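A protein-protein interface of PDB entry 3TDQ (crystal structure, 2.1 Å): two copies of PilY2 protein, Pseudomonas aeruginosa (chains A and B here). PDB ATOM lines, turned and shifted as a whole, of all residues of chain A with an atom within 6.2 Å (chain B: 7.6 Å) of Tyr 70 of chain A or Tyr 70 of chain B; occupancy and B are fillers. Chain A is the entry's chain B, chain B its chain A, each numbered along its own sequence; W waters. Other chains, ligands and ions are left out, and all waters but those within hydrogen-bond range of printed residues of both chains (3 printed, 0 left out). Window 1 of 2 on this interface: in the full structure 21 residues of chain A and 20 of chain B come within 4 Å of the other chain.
OE2 of Glu 8 of chain B sits at hydrogen-bond distance from OH of Tyr 70 of chain A, at 2.6 Å.
OE2 of Glu 8 of chain B is in hydrogen-bond range of N of Lys 73 of chain A, at 3.0 Å.
The guanidinium group (NE) of Arg 38 of chain B is in salt-bridge range of the side-chain carboxylate (OD1) of Asp 68 of chain A.
The backbone carbonyl oxygen (O) of Ile 69 of chain A is in hydrogen-bond range of the guanidinium group (NH2) of Arg 38 of chain B.
OH of Tyr 70 of chain A lies close to O of Tyr 55 of chain B (3.3 Å).
The side-chain amino group (NZ) of Lys 73 of chain A is in hydrogen-bond range of the side-chain hydroxyl (OG) of Ser 56 of chain B, 3.0 Å away.
OD2 of Asp 68 of chain B lies within salt-bridge range of NZ of Lys 73 of chain A, at 2.8 Å.
The side-chain hydroxyl (OH) of Tyr 70 of chain B lies within hydrogen-bond range of the side-chain carboxylate (OE2) of Glu 8 of chain A, at 2.7 Å.
The backbone carbonyl oxygen (O) of Tyr 55 of chain A lies close to the side-chain hydroxyl (OH) of Tyr 70 of chain B (3.4 Å).
The side-chain hydroxyl (OG) of Ser 56 of chain A is in hydrogen-bond range of the side-chain hydroxyl (OH) of Tyr 70 of chain B (3.4 Å).
N of Lys 73 of chain B sits at hydrogen-bond distance from OE2 of Glu 8 of chain A (2.9 Å).
NZ of Lys 73 of chain B is in hydrogen-bond range of OG of Ser 56 of chain A, at 2.9 Å.
The side-chain carboxylate of Asp 68 of chain A lies within salt-bridge range of the side-chain amino group of Lys 73 of chain B (2.7 Å).
The side-chain amide nitrogen (NE2) of Gln 78 of chain B lies within hydrogen-bond range of the side-chain carboxylate (OE1) of Glu 8 of chain A, 3.1 Å away.
N of Tyr 55 of chain B is in hydrogen-bond range of O of Gly 9 of chain B (2.9 Å).
The backbone carbonyl oxygen of Ser 56 of chain B is in hydrogen-bond range of the backbone NH of Thr 67 of chain B (2.9 Å).
N of Gly 9 of chain A lies within hydrogen-bond range of O of Tyr 55 of chain A, 2.9 Å away.
OG of Ser 54 of chain A lies within hydrogen-bond range of NE2 of His 72 of chain A (2.6 Å).
OE2 of Glu 8 of chain A touches CA of His 72 of chain B, 3.5 Å away.
Asp 68 of chain A touches Tyr 70 of chain B.
Tyr 70 of chain A touches Arg 38 of chain B (CA to NH2, 3.8 Å).
CE2 of Tyr 70 of chain A touches CB of Ser 54 of chain B, 3.8 Å away.
Tyr 70 of chain A touches Ser 56 of chain B (OH to OG, 3.5 Å).
Tyr 70 of chain A touches Asp 68 of chain B (CE1 to OD2, 3.6 Å).
His 72 of chain A touches Glu 8 of chain B.
Of the printed residues of chain B, Ser 54 of chain A touches Tyr 70.
Of the printed residues of chain B, Tyr 55 of chain A touches Tyr 70.
Of the printed residues of chain B, Ile 69 of chain A touches Arg 38 (3.0 Å).
Of chain B, only Glu 8, Arg 38, Ser 54, Tyr 55, Ser 56, Asp 68 and Tyr 70 come within 4 Å of Tyr 70 of chain A.
Phe 7 of chain B touches none of the printed residues of chain A.
Printed residues of chain A within 4 Å of Glu 8 of chain B: Tyr 70, His 72 and Lys 73.
The nearest printed residue of chain B that does not touch Asp 68 of chain A is Ile 71 of chain B (4.6 Å).
Printed residues of chain B that touch a printed residue of chain A: Glu 8, Arg 38, Ser 54, Tyr 55, Ser 56, Asp 68, Tyr 70, His 72, Lys 73 and Gln 78.
Of the 13 printed residues of chain A, 9 touch a printed residue of chain B.
Among the printed residues, Asp or Glu carboxylates within 4 Å of a Lys or Arg side-chain nitrogen of the other chain: Asp 68 of chain A with Arg 38 of chain B (2.8 Å), Asp 68 of chain A with Lys 73 of chain B (2.7 Å) and Lys 73 of chain A with Asp 68 of chain B (2.8 Å).
Glu 8 of chain A touches Tyr 70 of chain B, and with the chains exchanged Tyr 70 of chain A touches Glu 8 of chain B.
Tyr 55 of chain A touches Tyr 70 of chain B, and with the chains exchanged Tyr 70 of chain A touches Tyr 55 of chain B.
Tyr 70 of chain B touches its own counterpart, Tyr 70 of chain A.
Water W1 lies within hydrogen-bond range of the side-chain carboxylate of Asp 68 of chain A (2.7 Å) and the backbone NH of Ile 71 of chain B (2.9 Å).
Water W3 lies within hydrogen-bond range of the side-chain amide oxygen (OE1) of Gln 78 of chain B (2.9 Å) and the backbone carbonyl oxygen (O) of Glu 8 of chain A (3.3 Å).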
ATOM      1  N   GLU A   8     -17.494  18.937  31.452  1.00  0.00           N
ATOM      2  CA  GLU A   8     -18.897  19.300  31.404  1.00  0.00           C
ATOM      3  C   GLU A   8     -19.729  18.198  32.048  1.00  0.00           C
ATOM      4  O   GLU A   8     -19.418  17.026  31.879  1.00  0.00           O
ATOM      5  CB  GLU A   8     -19.341  19.560  29.956  1.00  0.00           C
ATOM      6  CG  GLU A   8     -20.820  19.908  29.843  1.00  0.00           C
ATOM      7  CD  GLU A   8     -21.295  20.365  28.482  1.00  0.00           C
ATOM      8  OE1 GLU A   8     -21.069  19.626  27.501  1.00  0.00           O
ATOM      9  OE2 GLU A   8     -21.909  21.451  28.400  1.00  0.00           O
ATOM     10  N   GLY A   9     -20.789  18.587  32.747  1.00  0.00           N
ATOM     11  CA  GLY A   9     -21.702  17.635  33.351  1.00  0.00           C
ATOM     12  C   GLY A   9     -23.099  18.200  33.489  1.00  0.00           C
ATOM     13  O   GLY A   9     -23.379  19.325  33.073  1.00  0.00           O
ATOM     14  N   VAL A  52     -31.967  21.879  38.748  1.00  0.00           N
ATOM     15  CA  VAL A  52     -31.488  20.937  37.742  1.00  0.00           C
ATOM     16  C   VAL A  52     -30.536  21.754  36.883  1.00  0.00           C
ATOM     17  O   VAL A  52     -30.925  22.811  36.389  1.00  0.00           O
ATOM     18  CB  VAL A  52     -32.638  20.264  36.943  1.00  0.00           C
ATOM     19  CG1 VAL A  52     -32.089  19.485  35.745  1.00  0.00           C
ATOM     20  CG2 VAL A  52     -33.477  19.355  37.842  1.00  0.00           C
ATOM     21  N   VAL A  53     -29.273  21.322  36.767  1.00  0.00           N
ATOM     22  CA  VAL A  53     -28.265  22.150  36.105  1.00  0.00           C
ATOM     23  C   VAL A  53     -27.427  21.437  35.051  1.00  0.00           C
ATOM     24  O   VAL A  53     -27.215  20.227  35.125  1.00  0.00           O
ATOM     25  CB  VAL A  53     -27.297  22.747  37.173  1.00  0.00           C
ATOM     26  CG1 VAL A  53     -27.974  23.839  38.004  1.00  0.00           C
ATOM     27  CG2 VAL A  53     -26.692  21.655  38.096  1.00  0.00           C
ATOM     28  N   SER A  54     -26.942  22.219  34.078  1.00  0.00           N
ATOM     29  CA  SER A  54     -25.922  21.861  33.084  1.00  0.00           C
ATOM     30  C   SER A  54     -24.758  22.756  33.424  1.00  0.00           C
ATOM     31  O   SER A  54     -24.999  23.918  33.760  1.00  0.00           O
ATOM     32  CB  SER A  54     -26.421  22.078  31.657  1.00  0.00           C
ATOM     33  OG  SER A  54     -27.419  21.117  31.364  1.00  0.00           O
ATOM     34  N   TYR A  55     -23.530  22.229  33.474  1.00  0.00           N
ATOM     35  CA  TYR A  55     -22.401  23.068  33.878  1.00  0.00           C
ATOM     36  C   TYR A  55     -21.113  22.643  33.192  1.00  0.00           C
ATOM     37  O   TYR A  55     -20.984  21.511  32.741  1.00  0.00           O
ATOM     38  CB  TYR A  55     -22.207  23.056  35.425  1.00  0.00           C
ATOM     39  CG  TYR A  55     -22.149  21.655  35.995  1.00  0.00           C
ATOM     40  CD1 TYR A  55     -20.941  20.966  36.079  1.00  0.00           C
ATOM     41  CD2 TYR A  55     -23.315  20.970  36.338  1.00  0.00           C
ATOM     42  CE1 TYR A  55     -20.885  19.654  36.543  1.00  0.00           C
ATOM     43  CE2 TYR A  55     -23.273  19.648  36.772  1.00  0.00           C
ATOM     44  CZ  TYR A  55     -22.055  18.998  36.882  1.00  0.00           C
ATOM     45  OH  TYR A  55     -22.016  17.700  37.336  1.00  0.00           O
ATOM     46  N   SER A  56     -20.159  23.556  33.130  1.00  0.00           N
ATOM     47  CA  SER A  56     -18.854  23.272  32.534  1.00  0.00           C
ATOM     48  C   SER A  56     -17.807  24.075  33.274  1.00  0.00           C
ATOM     49  O   SER A  56     -18.144  25.039  33.975  1.00  0.00           O
ATOM     50  CB  SER A  56     -18.847  23.556  31.036  1.00  0.00           C
ATOM     51  OG  SER A  56     -19.201  24.894  30.742  1.00  0.00           O
ATOM     52  N   ASP A  68     -19.251  28.020  34.077  1.00  0.00           N
ATOM     53  CA  ASP A  68     -20.490  28.259  33.332  1.00  0.00           C
ATOM     54  C   ASP A  68     -21.575  27.307  33.852  1.00  0.00           C
ATOM     55  O   ASP A  68     -21.338  26.104  33.909  1.00  0.00           O
ATOM     56  CB  ASP A  68     -20.236  28.056  31.807  1.00  0.00           C
ATOM     57  CG  ASP A  68     -21.343  28.574  30.891  1.00  0.00           C
ATOM     58  OD1 ASP A  68     -22.310  29.160  31.404  1.00  0.00           O
ATOM     59  OD2 ASP A  68     -21.238  28.386  29.652  1.00  0.00           O
ATOM     60  N   ILE A  69     -22.740  27.828  34.268  1.00  0.00           N
ATOM     61  CA  ILE A  69     -23.807  26.951  34.760  1.00  0.00           C
ATOM     62  C   ILE A  69     -25.167  27.486  34.318  1.00  0.00           C
ATOM     63  O   ILE A  69     -25.404  28.693  34.355  1.00  0.00           O
ATOM     64  CB  ILE A  69     -23.696  26.719  36.314  1.00  0.00           C
ATOM     65  CG1 ILE A  69     -24.713  25.677  36.848  1.00  0.00           C
ATOM     66  CG2 ILE A  69     -23.742  28.009  37.116  1.00  0.00           C
ATOM     67  CD1 ILE A  69     -24.309  25.011  38.273  1.00  0.00           C
ATOM     68  N   TYR A  70     -26.068  26.573  33.919  1.00  0.00           N
ATOM     69  CA  TYR A  70     -27.414  26.903  33.465  1.00  0.00           C
ATOM     70  C   TYR A  70     -28.453  26.141  34.286  1.00  0.00           C
ATOM     71  O   TYR A  70     -28.336  24.933  34.445  1.00  0.00           O
ATOM     72  CB  TYR A  70     -27.553  26.578  31.961  1.00  0.00           C
ATOM     73  CG  TYR A  70     -28.953  26.751  31.393  1.00  0.00           C
ATOM     74  CD1 TYR A  70     -29.381  27.984  30.896  1.00  0.00           C
ATOM     75  CD2 TYR A  70     -29.821  25.671  31.288  1.00  0.00           C
ATOM     76  CE1 TYR A  70     -30.666  28.150  30.374  1.00  0.00           C
ATOM     77  CE2 TYR A  70     -31.112  25.824  30.763  1.00  0.00           C
ATOM     78  CZ  TYR A  70     -31.525  27.067  30.310  1.00  0.00           C
ATOM     79  OH  TYR A  70     -32.779  27.227  29.801  1.00  0.00           O
ATOM     80  N   ILE A  71     -29.482  26.849  34.787  1.00  0.00           N
ATOM     81  CA  ILE A  71     -30.558  26.216  35.545  1.00  0.00           C
ATOM     82  C   ILE A  71     -31.684  25.883  34.582  1.00  0.00           C
ATOM     83  O   ILE A  71     -32.189  26.779  33.894  1.00  0.00           O
ATOM     84  CB  ILE A  71     -31.043  27.086  36.740  1.00  0.00           C
ATOM     85  CG1 ILE A  71     -29.893  27.382  37.747  1.00  0.00           C
ATOM     86  CG2 ILE A  71     -32.255  26.445  37.441  1.00  0.00           C
ATOM     87  CD1 ILE A  71     -30.150  28.665  38.620  1.00  0.00           C
ATOM     88  N   HIS A  72     -32.059  24.588  34.512  1.00  0.00           N
ATOM     89  CA  HIS A  72     -33.168  24.098  33.675  1.00  0.00           C
ATOM     90  C   HIS A  72     -34.461  24.562  34.336  1.00  0.00           C
ATOM     91  O   HIS A  72     -34.693  24.246  35.490  1.00  0.00           O
ATOM     92  CB  HIS A  72     -33.074  22.578  33.514  1.00  0.00           C
ATOM     93  CG  HIS A  72     -31.884  22.165  32.707  1.00  0.00           C
ATOM     94  ND1 HIS A  72     -31.963  22.015  31.338  1.00  0.00           N
ATOM     95  CD2 HIS A  72     -30.597  21.995  33.090  1.00  0.00           C
ATOM     96  CE1 HIS A  72     -30.741  21.698  30.942  1.00  0.00           C
ATOM     97  NE2 HIS A  72     -29.889  21.664  31.968  1.00  0.00           N
ATOM     98  N   LYS A  73     -35.204  25.458  33.694  1.00  0.00           N
ATOM     99  CA  LYS A  73     -36.359  26.109  34.328  1.00  0.00           C
ATOM    100  C   LYS A  73     -37.556  25.174  34.580  1.00  0.00           C
ATOM    101  O   LYS A  73     -38.147  25.246  35.666  1.00  0.00           O
ATOM    102  CB  LYS A  73     -36.807  27.352  33.527  1.00  0.00           C
ATOM    103  CG  LYS A  73     -35.652  28.273  33.056  1.00  0.00           C
ATOM    104  CD  LYS A  73     -34.847  28.908  34.192  1.00  0.00           C
ATOM    105  CE  LYS A  73     -33.813  29.922  33.726  1.00  0.00           C
ATOM    106  NZ  LYS A  73     -32.758  29.331  32.831  1.00  0.00           N
ATOM    107  N   PHE B   7     -40.734  30.714  28.286  1.00  0.00           N
ATOM    108  CA  PHE B   7     -40.513  29.513  27.478  1.00  0.00           C
ATOM    109  C   PHE B   7     -39.102  28.981  27.726  1.00  0.00           C
ATOM    110  O   PHE B   7     -38.222  29.723  28.165  1.00  0.00           O
ATOM    111  CB  PHE B   7     -40.747  29.807  25.975  1.00  0.00           C
ATOM    112  CG  PHE B   7     -39.651  30.643  25.374  1.00  0.00           C
ATOM    113  CD1 PHE B   7     -39.676  32.038  25.477  1.00  0.00           C
ATOM    114  CD2 PHE B   7     -38.572  30.034  24.735  1.00  0.00           C
ATOM    115  CE1 PHE B   7     -38.646  32.804  24.939  1.00  0.00           C
ATOM    116  CE2 PHE B   7     -37.541  30.789  24.212  1.00  0.00           C
ATOM    117  CZ  PHE B   7     -37.588  32.174  24.302  1.00  0.00           C
ATOM    118  N   GLU B   8     -38.880  27.716  27.384  1.00  0.00           N
ATOM    119  CA  GLU B   8     -37.583  27.080  27.466  1.00  0.00           C
ATOM    120  C   GLU B   8     -37.479  26.055  26.349  1.00  0.00           C
ATOM    121  O   GLU B   8     -38.457  25.386  26.023  1.00  0.00           O
ATOM    122  CB  GLU B   8     -37.362  26.422  28.840  1.00  0.00           C
ATOM    123  CG  GLU B   8     -36.026  25.704  28.956  1.00  0.00           C
ATOM    124  CD  GLU B   8     -35.674  25.235  30.352  1.00  0.00           C
ATOM    125  OE1 GLU B   8     -36.529  24.610  31.019  1.00  0.00           O
ATOM    126  OE2 GLU B   8     -34.542  25.529  30.793  1.00  0.00           O
ATOM    127  N   GLY B   9     -36.291  25.922  25.789  1.00  0.00           N
ATOM    128  CA  GLY B   9     -36.038  24.926  24.755  1.00  0.00           C
ATOM    129  C   GLY B   9     -34.579  24.556  24.652  1.00  0.00           C
ATOM    130  O   GLY B   9     -33.752  25.006  25.452  1.00  0.00           O
ATOM    131  N   ALA B  10     -34.261  23.728  23.654  1.00  0.00           N
ATOM    132  CA  ALA B  10     -32.901  23.301  23.341  1.00  0.00           C
ATOM    133  C   ALA B  10     -32.802  22.989  21.865  1.00  0.00           C
ATOM    134  O   ALA B  10     -33.780  22.569  21.261  1.00  0.00           O
ATOM    135  CB  ALA B  10     -32.499  22.091  24.175  1.00  0.00           C
ATOM    136  N   GLY B  11     -31.649  23.259  21.276  1.00  0.00           N
ATOM    137  CA  GLY B  11     -31.452  22.988  19.859  1.00  0.00           C
ATOM    138  C   GLY B  11     -30.067  23.325  19.368  1.00  0.00           C
ATOM    139  O   GLY B  11     -29.116  23.375  20.147  1.00  0.00           O
ATOM    140  N   ARG B  38     -23.449  36.709  29.802  1.00  0.00           N
ATOM    141  CA  ARG B  38     -22.872  35.613  30.563  1.00  0.00           C
ATOM    142  C   ARG B  38     -21.373  35.919  30.690  1.00  0.00           C
ATOM    143  O   ARG B  38     -20.709  36.195  29.684  1.00  0.00           O
ATOM    144  CB  ARG B  38     -23.159  34.266  29.853  1.00  0.00           C
ATOM    145  CG  ARG B  38     -23.117  33.020  30.735  1.00  0.00           C
ATOM    146  CD  ARG B  38     -23.700  31.784  30.000  1.00  0.00           C
ATOM    147  NE  ARG B  38     -24.482  30.925  30.900  1.00  0.00           N
ATOM    148  CZ  ARG B  38     -25.787  31.038  31.080  1.00  0.00           C
ATOM    149  NH1 ARG B  38     -26.493  31.895  30.351  1.00  0.00           N
ATOM    150  NH2 ARG B  38     -26.405  30.282  31.969  1.00  0.00           N
ATOM    151  N   SER B  43     -24.192  37.186  25.057  1.00  0.00           N
ATOM    152  CA  SER B  43     -24.291  35.829  24.476  1.00  0.00           C
ATOM    153  C   SER B  43     -24.456  35.860  22.948  1.00  0.00           C
ATOM    154  O   SER B  43     -24.105  34.896  22.273  1.00  0.00           O
ATOM    155  CB  SER B  43     -25.452  35.060  25.099  1.00  0.00           C
ATOM    156  OG  SER B  43     -25.299  34.975  26.509  1.00  0.00           O
ATOM    157  N   VAL B  47     -22.581  32.686  20.723  1.00  0.00           N
ATOM    158  CA  VAL B  47     -23.220  31.638  19.923  1.00  0.00           C
ATOM    159  C   VAL B  47     -22.743  31.749  18.471  1.00  0.00           C
ATOM    160  O   VAL B  47     -22.438  32.839  17.994  1.00  0.00           O
ATOM    161  CB  VAL B  47     -24.769  31.599  20.026  1.00  0.00           C
ATOM    162  CG1 VAL B  47     -25.206  31.242  21.444  1.00  0.00           C
ATOM    163  CG2 VAL B  47     -25.422  32.901  19.550  1.00  0.00           C
ATOM    164  N   SER B  51     -23.465  25.819  17.249  1.00  0.00           N
ATOM    165  CA  SER B  51     -23.544  25.772  18.721  1.00  0.00           C
ATOM    166  C   SER B  51     -24.751  24.959  19.151  1.00  0.00           C
ATOM    167  O   SER B  51     -25.846  25.125  18.593  1.00  0.00           O
ATOM    168  CB  SER B  51     -23.632  27.170  19.340  1.00  0.00           C
ATOM    169  OG  SER B  51     -22.502  27.973  19.053  1.00  0.00           O
ATOM    170  N   VAL B  52     -24.552  24.068  20.129  1.00  0.00           N
ATOM    171  CA  VAL B  52     -25.640  23.267  20.676  1.00  0.00           C
ATOM    172  C   VAL B  52     -26.063  24.033  21.925  1.00  0.00           C
ATOM    173  O   VAL B  52     -25.206  24.343  22.752  1.00  0.00           O
ATOM    174  CB  VAL B  52     -25.222  21.795  20.934  1.00  0.00           C
ATOM    175  CG1 VAL B  52     -26.274  21.059  21.760  1.00  0.00           C
ATOM    176  CG2 VAL B  52     -24.938  21.068  19.622  1.00  0.00           C
ATOM    177  N   VAL B  53     -27.348  24.404  22.031  1.00  0.00           N
ATOM    178  CA  VAL B  53     -27.772  25.304  23.126  1.00  0.00           C
ATOM    179  C   VAL B  53     -29.007  24.873  23.897  1.00  0.00           C
ATOM    180  O   VAL B  53     -29.862  24.181  23.369  1.00  0.00           O
ATOM    181  CB  VAL B  53     -28.033  26.726  22.556  1.00  0.00           C
ATOM    182  CG1 VAL B  53     -26.723  27.430  22.175  1.00  0.00           C
ATOM    183  CG2 VAL B  53     -29.035  26.699  21.373  1.00  0.00           C
ATOM    184  N   SER B  54     -29.079  25.316  25.165  1.00  0.00           N
ATOM    185  CA  SER B  54     -30.237  25.256  26.060  1.00  0.00           C
ATOM    186  C   SER B  54     -30.575  26.706  26.302  1.00  0.00           C
ATOM    187  O   SER B  54     -29.647  27.510  26.474  1.00  0.00           O
ATOM    188  CB  SER B  54     -29.927  24.520  27.357  1.00  0.00           C
ATOM    189  OG  SER B  54     -29.766  23.140  27.088  1.00  0.00           O
ATOM    190  N   TYR B  55     -31.862  27.086  26.236  1.00  0.00           N
ATOM    191  CA  TYR B  55     -32.187  28.509  26.385  1.00  0.00           C
ATOM    192  C   TYR B  55     -33.549  28.707  27.021  1.00  0.00           C
ATOM    193  O   TYR B  55     -34.402  27.818  26.974  1.00  0.00           O
ATOM    194  CB  TYR B  55     -32.125  29.242  25.011  1.00  0.00           C
ATOM    195  CG  TYR B  55     -32.935  28.550  23.938  1.00  0.00           C
ATOM    196  CD1 TYR B  55     -34.282  28.850  23.751  1.00  0.00           C
ATOM    197  CD2 TYR B  55     -32.385  27.518  23.178  1.00  0.00           C
ATOM    198  CE1 TYR B  55     -35.053  28.166  22.814  1.00  0.00           C
ATOM    199  CE2 TYR B  55     -33.156  26.809  22.254  1.00  0.00           C
ATOM    200  CZ  TYR B  55     -34.486  27.140  22.073  1.00  0.00           C
ATOM    201  OH  TYR B  55     -35.246  26.459  21.155  1.00  0.00           O
ATOM    202  N   SER B  56     -33.763  29.895  27.579  1.00  0.00           N
ATOM    203  CA  SER B  56     -35.050  30.251  28.166  1.00  0.00           C
ATOM    204  C   SER B  56     -35.267  31.733  28.002  1.00  0.00           C
ATOM    205  O   SER B  56     -34.315  32.473  27.747  1.00  0.00           O
ATOM    206  CB  SER B  56     -35.122  29.834  29.637  1.00  0.00           C
ATOM    207  OG  SER B  56     -34.088  30.422  30.404  1.00  0.00           O
ATOM    208  N   GLY B  57     -36.519  32.157  28.096  1.00  0.00           N
ATOM    209  CA  GLY B  57     -36.838  33.562  27.941  1.00  0.00           C
ATOM    210  C   GLY B  57     -38.292  33.889  28.166  1.00  0.00           C
ATOM    211  O   GLY B  57     -39.035  33.100  28.756  1.00  0.00           O
ATOM    212  N   ILE B  66     -34.795  35.613  24.226  1.00  0.00           N
ATOM    213  CA  ILE B  66     -33.957  34.708  25.011  1.00  0.00           C
ATOM    214  C   ILE B  66     -33.235  35.563  26.054  1.00  0.00           C
ATOM    215  O   ILE B  66     -32.493  36.489  25.690  1.00  0.00           O
ATOM    216  CB  ILE B  66     -32.985  33.875  24.118  1.00  0.00           C
ATOM    217  CG1 ILE B  66     -33.765  32.824  23.284  1.00  0.00           C
ATOM    218  CG2 ILE B  66     -31.900  33.202  24.998  1.00  0.00           C
ATOM    219  CD1 ILE B  66     -32.932  32.086  22.204  1.00  0.00           C
ATOM    220  N   THR B  67     -33.467  35.261  27.344  1.00  0.00           N
ATOM    221  CA  THR B  67     -32.840  36.010  28.442  1.00  0.00           C
ATOM    222  C   THR B  67     -31.746  35.177  29.112  1.00  0.00           C
ATOM    223  O   THR B  67     -31.012  35.700  29.946  1.00  0.00           O
ATOM    224  CB  THR B  67     -33.895  36.471  29.474  1.00  0.00           C
ATOM    225  OG1 THR B  67     -34.549  35.315  29.988  1.00  0.00           O
ATOM    226  CG2 THR B  67     -34.918  37.433  28.873  1.00  0.00           C
ATOM    227  N   ASP B  68     -31.616  33.897  28.723  1.00  0.00           N
ATOM    228  CA  ASP B  68     -30.622  32.974  29.299  1.00  0.00           C
ATOM    229  C   ASP B  68     -30.274  31.904  28.278  1.00  0.00           C
ATOM    230  O   ASP B  68     -31.176  31.225  27.778  1.00  0.00           O
ATOM    231  CB  ASP B  68     -31.185  32.320  30.599  1.00  0.00           C
ATOM    232  CG  ASP B  68     -30.162  31.583  31.467  1.00  0.00           C
ATOM    233  OD1 ASP B  68     -28.964  31.604  31.128  1.00  0.00           O
ATOM    234  OD2 ASP B  68     -30.565  31.007  32.501  1.00  0.00           O
ATOM    235  N   ILE B  69     -28.992  31.778  27.916  1.00  0.00           N
ATOM    236  CA  ILE B  69     -28.618  30.751  26.929  1.00  0.00           C
ATOM    237  C   ILE B  69     -27.268  30.128  27.311  1.00  0.00           C
ATOM    238  O   ILE B  69     -26.327  30.838  27.662  1.00  0.00           O
ATOM    239  CB  ILE B  69     -28.658  31.294  25.469  1.00  0.00           C
ATOM    240  CG1 ILE B  69     -28.418  30.171  24.418  1.00  0.00           C
ATOM    241  CG2 ILE B  69     -27.754  32.530  25.273  1.00  0.00           C
ATOM    242  CD1 ILE B  69     -28.929  30.531  22.943  1.00  0.00           C
ATOM    243  N   TYR B  70     -27.194  28.788  27.218  1.00  0.00           N
ATOM    244  CA  TYR B  70     -26.015  28.018  27.574  1.00  0.00           C
ATOM    245  C   TYR B  70     -25.530  27.205  26.374  1.00  0.00           C
ATOM    246  O   TYR B  70     -26.317  26.504  25.747  1.00  0.00           O
ATOM    247  CB  TYR B  70     -26.338  27.100  28.771  1.00  0.00           C
ATOM    248  CG  TYR B  70     -25.236  26.130  29.150  1.00  0.00           C
ATOM    249  CD1 TYR B  70     -24.241  26.492  30.061  1.00  0.00           C
ATOM    250  CD2 TYR B  70     -25.233  24.821  28.667  1.00  0.00           C
ATOM    251  CE1 TYR B  70     -23.242  25.588  30.440  1.00  0.00           C
ATOM    252  CE2 TYR B  70     -24.244  23.910  29.044  1.00  0.00           C
ATOM    253  CZ  TYR B  70     -23.247  24.299  29.926  1.00  0.00           C
ATOM    254  OH  TYR B  70     -22.256  23.399  30.262  1.00  0.00           O
ATOM    255  N   ILE B  71     -24.228  27.279  26.083  1.00  0.00           N
ATOM    256  CA  ILE B  71     -23.627  26.509  24.989  1.00  0.00           C
ATOM    257  C   ILE B  71     -23.098  25.204  25.571  1.00  0.00           C
ATOM    258  O   ILE B  71     -22.285  25.228  26.493  1.00  0.00           O
ATOM    259  CB  ILE B  71     -22.528  27.330  24.256  1.00  0.00           C
ATOM    260  CG1 ILE B  71     -23.115  28.649  23.639  1.00  0.00           C
ATOM    261  CG2 ILE B  71     -21.822  26.470  23.181  1.00  0.00           C
ATOM    262  CD1 ILE B  71     -22.046  29.791  23.370  1.00  0.00           C
ATOM    263  N   HIS B  72     -23.580  24.073  25.049  1.00  0.00           N
ATOM    264  CA  HIS B  72     -23.134  22.735  25.436  1.00  0.00           C
ATOM    265  C   HIS B  72     -21.733  22.506  24.889  1.00  0.00           C
ATOM    266  O   HIS B  72     -21.485  22.734  23.696  1.00  0.00           O
ATOM    267  CB  HIS B  72     -24.116  21.674  24.932  1.00  0.00           C
ATOM    268  CG  HIS B  72     -25.433  21.741  25.628  1.00  0.00           C
ATOM    269  ND1 HIS B  72     -25.689  20.987  26.755  1.00  0.00           N
ATOM    270  CD2 HIS B  72     -26.486  22.556  25.403  1.00  0.00           C
ATOM    271  CE1 HIS B  72     -26.911  21.329  27.151  1.00  0.00           C
ATOM    272  NE2 HIS B  72     -27.434  22.256  26.354  1.00  0.00           N
ATOM    273  N   LYS B  73     -20.818  22.058  25.762  1.00  0.00           N
ATOM    274  CA  LYS B  73     -19.421  21.827  25.376  1.00  0.00           C
ATOM    275  C   LYS B  73     -19.205  20.369  25.013  1.00  0.00           C
ATOM    276  O   LYS B  73     -18.595  19.617  25.769  1.00  0.00           O
ATOM    277  CB  LYS B  73     -18.454  22.274  26.490  1.00  0.00           C
ATOM    278  CG  LYS B  73     -18.253  23.782  26.474  1.00  0.00           C
ATOM    279  CD  LYS B  73     -19.060  24.356  27.546  1.00  0.00           C
ATOM    280  CE  LYS B  73     -19.350  25.825  27.470  1.00  0.00           C
ATOM    281  NZ  LYS B  73     -20.472  26.093  28.443  1.00  0.00           N
ATOM    282  N   GLN B  78     -16.628  14.507  29.079  1.00  0.00           N
ATOM    283  CA  GLN B  78     -17.951  14.476  29.693  1.00  0.00           C
ATOM    284  C   GLN B  78     -17.995  13.667  30.977  1.00  0.00           C
ATOM    285  O   GLN B  78     -17.597  12.519  30.963  1.00  0.00           O
ATOM    286  CB  GLN B  78     -18.967  13.907  28.688  1.00  0.00           C
ATOM    287  CG  GLN B  78     -19.134  14.766  27.418  1.00  0.00           C
ATOM    288  CD  GLN B  78     -19.812  16.087  27.684  1.00  0.00           C
ATOM    289  OE1 GLN B  78     -20.751  16.197  28.483  1.00  0.00           O
ATOM    290  NE2 GLN B  78     -19.317  17.130  27.049  1.00  0.00           N
HETATM  291  O   HOH W   1     -22.595  29.238  27.524  1.00  0.00           O
HETATM  292  O   HOH W   2     -29.278  29.724  34.355  1.00  0.00           O
HETATM  293  O   HOH W   3     -21.687  14.833  30.904  1.00  0.00           O
